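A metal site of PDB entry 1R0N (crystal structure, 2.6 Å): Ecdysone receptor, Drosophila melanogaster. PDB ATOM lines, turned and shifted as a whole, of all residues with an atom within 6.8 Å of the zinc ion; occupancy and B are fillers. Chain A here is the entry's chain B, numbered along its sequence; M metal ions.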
ATOM      1  N   CYS A  44      -6.242  -6.840   4.821  1.00  0.00           N
ATOM      2  CA  CYS A  44      -6.476  -6.476   3.432  1.00  0.00           C
ATOM      3  C   CYS A  44      -6.428  -4.944   3.297  1.00  0.00           C
ATOM      4  O   CYS A  44      -7.102  -4.209   4.035  1.00  0.00           O
ATOM      5  CB  CYS A  44      -7.841  -7.034   3.015  1.00  0.00           C
ATOM      6  SG  CYS A  44      -8.407  -6.642   1.360  1.00  0.00           S
ATOM      7  N   CYS A  45      -5.595  -4.487   2.351  1.00  0.00           N
ATOM      8  CA  CYS A  45      -5.366  -3.062   2.091  1.00  0.00           C
ATOM      9  C   CYS A  45      -6.550  -2.350   1.448  1.00  0.00           C
ATOM     10  O   CYS A  45      -7.180  -2.869   0.540  1.00  0.00           O
ATOM     11  CB  CYS A  45      -4.134  -2.909   1.191  1.00  0.00           C
ATOM     12  SG  CYS A  45      -3.657  -1.189   0.810  1.00  0.00           S
ATOM     13  N   LYS A  46      -6.848  -1.142   1.941  1.00  0.00           N
ATOM     14  CA  LYS A  46      -7.962  -0.338   1.424  1.00  0.00           C
ATOM     15  C   LYS A  46      -7.571   0.365   0.138  1.00  0.00           C
ATOM     16  O   LYS A  46      -8.206   0.214  -0.902  1.00  0.00           O
ATOM     17  CB  LYS A  46      -8.398   0.715   2.450  1.00  0.00           C
ATOM     18  CG  LYS A  46      -9.103   0.162   3.680  1.00  0.00           C
ATOM     19  CD  LYS A  46     -10.445  -0.459   3.324  1.00  0.00           C
ATOM     20  CE  LYS A  46     -11.092  -1.213   4.506  1.00  0.00           C
ATOM     21  NZ  LYS A  46     -12.374  -1.927   4.157  1.00  0.00           N
ATOM     22  N   PHE A  47      -6.505   1.145   0.227  1.00  0.00           N
ATOM     23  CA  PHE A  47      -5.982   1.895  -0.908  1.00  0.00           C
ATOM     24  C   PHE A  47      -5.274   0.900  -1.804  1.00  0.00           C
ATOM     25  O   PHE A  47      -5.787  -0.192  -2.035  1.00  0.00           O
ATOM     26  CB  PHE A  47      -5.029   2.938  -0.356  1.00  0.00           C
ATOM     27  CG  PHE A  47      -5.260   3.221   1.097  1.00  0.00           C
ATOM     28  CD1 PHE A  47      -4.730   2.371   2.092  1.00  0.00           C
ATOM     29  CD2 PHE A  47      -6.102   4.265   1.502  1.00  0.00           C
ATOM     30  CE1 PHE A  47      -5.040   2.546   3.444  1.00  0.00           C
ATOM     31  CE2 PHE A  47      -6.422   4.447   2.858  1.00  0.00           C
ATOM     32  CZ  PHE A  47      -5.896   3.584   3.823  1.00  0.00           C
ATOM     33  N   GLY A  48      -4.103   1.256  -2.304  1.00  0.00           N
ATOM     34  CA  GLY A  48      -3.371   0.334  -3.150  1.00  0.00           C
ATOM     35  C   GLY A  48      -2.254  -0.282  -2.328  1.00  0.00           C
ATOM     36  O   GLY A  48      -1.366   0.428  -1.858  1.00  0.00           O
ATOM     37  N   ARG A  49      -2.323  -1.597  -2.127  1.00  0.00           N
ATOM     38  CA  ARG A  49      -1.316  -2.330  -1.350  1.00  0.00           C
ATOM     39  C   ARG A  49       0.103  -1.869  -1.723  1.00  0.00           C
ATOM     40  O   ARG A  49       0.833  -2.592  -2.389  1.00  0.00           O
ATOM     41  CB  ARG A  49      -1.461  -3.817  -1.660  1.00  0.00           C
ATOM     42  CG  ARG A  49      -2.835  -4.191  -2.217  1.00  0.00           C
ATOM     43  CD  ARG A  49      -2.948  -5.699  -2.465  1.00  0.00           C
ATOM     44  NE  ARG A  49      -3.990  -6.295  -1.634  1.00  0.00           N
ATOM     45  CZ  ARG A  49      -4.177  -7.605  -1.463  1.00  0.00           C
ATOM     46  NH1 ARG A  49      -3.384  -8.474  -2.084  1.00  0.00           N
ATOM     47  NH2 ARG A  49      -5.156  -8.044  -0.672  1.00  0.00           N
ATOM     48  N   ALA A  50       0.484  -0.673  -1.271  1.00  0.00           N
ATOM     49  CA  ALA A  50       1.797  -0.137  -1.627  1.00  0.00           C
ATOM     50  C   ALA A  50       2.182   1.042  -0.738  1.00  0.00           C
ATOM     51  O   ALA A  50       3.143   1.777  -1.023  1.00  0.00           O
ATOM     52  CB  ALA A  50       1.791   0.286  -3.068  1.00  0.00           C
ATOM     53  N   CYS A  51       1.408   1.204   0.327  1.00  0.00           N
ATOM     54  CA  CYS A  51       1.586   2.258   1.307  1.00  0.00           C
ATOM     55  C   CYS A  51       2.979   2.289   1.892  1.00  0.00           C
ATOM     56  O   CYS A  51       3.489   1.261   2.308  1.00  0.00           O
ATOM     57  CB  CYS A  51       0.602   2.077   2.466  1.00  0.00           C
ATOM     58  SG  CYS A  51      -1.077   1.669   1.993  1.00  0.00           S
ATOM     59  N   GLU A  52       3.568   3.474   1.921  1.00  0.00           N
ATOM     60  CA  GLU A  52       4.880   3.667   2.514  1.00  0.00           C
ATOM     61  C   GLU A  52       4.648   3.875   4.014  1.00  0.00           C
ATOM     62  O   GLU A  52       3.705   4.547   4.416  1.00  0.00           O
ATOM     63  CB  GLU A  52       5.575   4.887   1.927  1.00  0.00           C
ATOM     64  CG  GLU A  52       6.068   4.714   0.506  1.00  0.00           C
ATOM     65  CD  GLU A  52       7.120   5.766   0.116  1.00  0.00           C
ATOM     66  OE1 GLU A  52       8.180   5.813   0.793  1.00  0.00           O
ATOM     67  OE2 GLU A  52       6.885   6.542  -0.855  1.00  0.00           O
ATOM     68  N   LYS A  60      -2.398   3.070   9.982  1.00  0.00           N
ATOM     69  CA  LYS A  60      -3.447   3.139   8.985  1.00  0.00           C
ATOM     70  C   LYS A  60      -3.539   1.946   8.035  1.00  0.00           C
ATOM     71  O   LYS A  60      -4.565   1.742   7.376  1.00  0.00           O
ATOM     72  CB  LYS A  60      -3.282   4.425   8.174  1.00  0.00           C
ATOM     73  CG  LYS A  60      -3.583   5.714   8.926  1.00  0.00           C
ATOM     74  CD  LYS A  60      -5.059   5.772   9.300  1.00  0.00           C
ATOM     75  CE  LYS A  60      -5.568   7.170   9.428  1.00  0.00           C
ATOM     76  NZ  LYS A  60      -7.024   7.093   9.653  1.00  0.00           N
ATOM     77  N   CYS A  61      -2.478   1.181   7.891  1.00  0.00           N
ATOM     78  CA  CYS A  61      -2.568   0.030   7.005  1.00  0.00           C
ATOM     79  C   CYS A  61      -1.907  -1.204   7.572  1.00  0.00           C
ATOM     80  O   CYS A  61      -0.706  -1.377   7.529  1.00  0.00           O
ATOM     81  CB  CYS A  61      -2.003   0.353   5.625  1.00  0.00           C
ATOM     82  SG  CYS A  61      -2.664  -0.803   4.403  1.00  0.00           S
ATOM     83  N   GLN A  62      -2.735  -2.062   8.130  1.00  0.00           N
ATOM     84  CA  GLN A  62      -2.261  -3.290   8.731  1.00  0.00           C
ATOM     85  C   GLN A  62      -1.658  -4.196   7.693  1.00  0.00           C
ATOM     86  O   GLN A  62      -0.576  -4.720   7.899  1.00  0.00           O
ATOM     87  CB  GLN A  62      -3.412  -3.961   9.483  1.00  0.00           C
ATOM     88  CG  GLN A  62      -3.704  -3.254  10.802  1.00  0.00           C
ATOM     89  CD  GLN A  62      -4.913  -3.800  11.549  1.00  0.00           C
ATOM     90  OE1 GLN A  62      -4.957  -3.757  12.779  1.00  0.00           O
ATOM     91  NE2 GLN A  62      -5.914  -4.294  10.816  1.00  0.00           N
ATOM     92  N   GLU A  63      -2.324  -4.385   6.578  1.00  0.00           N
ATOM     93  CA  GLU A  63      -1.734  -5.266   5.593  1.00  0.00           C
ATOM     94  C   GLU A  63      -0.320  -4.813   5.222  1.00  0.00           C
ATOM     95  O   GLU A  63       0.577  -5.641   5.120  1.00  0.00           O
ATOM     96  CB  GLU A  63      -2.551  -5.390   4.307  1.00  0.00           C
ATOM     97  CG  GLU A  63      -2.075  -6.628   3.553  1.00  0.00           C
ATOM     98  CD  GLU A  63      -2.226  -6.564   2.013  1.00  0.00           C
ATOM     99  OE1 GLU A  63      -1.696  -5.601   1.397  1.00  0.00           O
ATOM    100  OE2 GLU A  63      -2.828  -7.489   1.421  1.00  0.00           O
ATOM    101  N   CYS A  64      -0.117  -3.512   5.059  1.00  0.00           N
ATOM    102  CA  CYS A  64       1.212  -3.035   4.684  1.00  0.00           C
ATOM    103  C   CYS A  64       2.229  -2.954   5.799  1.00  0.00           C
ATOM    104  O   CYS A  64       3.437  -2.982   5.546  1.00  0.00           O
ATOM    105  CB  CYS A  64       1.123  -1.685   3.954  1.00  0.00           C
ATOM    106  SG  CYS A  64       0.482  -1.823   2.257  1.00  0.00           S
ATOM    107  N   ARG A  65       1.772  -2.847   7.034  1.00  0.00           N
ATOM    108  CA  ARG A  65       2.700  -2.820   8.147  1.00  0.00           C
ATOM    109  C   ARG A  65       3.290  -4.217   8.301  1.00  0.00           C
ATOM    110  O   ARG A  65       4.485  -4.370   8.558  1.00  0.00           O
ATOM    111  CB  ARG A  65       1.990  -2.403   9.417  1.00  0.00           C
ATOM    112  CG  ARG A  65       2.917  -2.205  10.585  1.00  0.00           C
ATOM    113  CD  ARG A  65       2.142  -1.664  11.715  1.00  0.00           C
ATOM    114  NE  ARG A  65       2.960  -1.278  12.874  1.00  0.00           N
ATOM    115  CZ  ARG A  65       2.445  -0.761  13.979  1.00  0.00           C
ATOM    116  NH1 ARG A  65       1.132  -0.589  14.073  1.00  0.00           N
ATOM    117  NH2 ARG A  65       3.230  -0.366  14.968  1.00  0.00           N
HETATM  118 ZN    ZN M   1      -1.478  -0.638   2.291  1.00  0.00          ZN
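Along chain A the residues within 4 Å of the zinc ion span positions 45 to 64.
SG of Cys 64 binds the zinc ion (2.3 Å). The side-chain sulfur (SG) of Cys 51 is bound to the zinc ion (2.4 Å). The zinc ion is bound by SG of Cys 61, 2.4 Å away. The zinc ion is bound by SG of Cys 45.
SG of Cys 64 lies close to N of Ala 50, 3.7 Å away. SG of Cys 45 lies close to N of Arg 49 (3.3 Å). SG of Cys 45 lies close to O of Phe 47 (3.7 Å).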
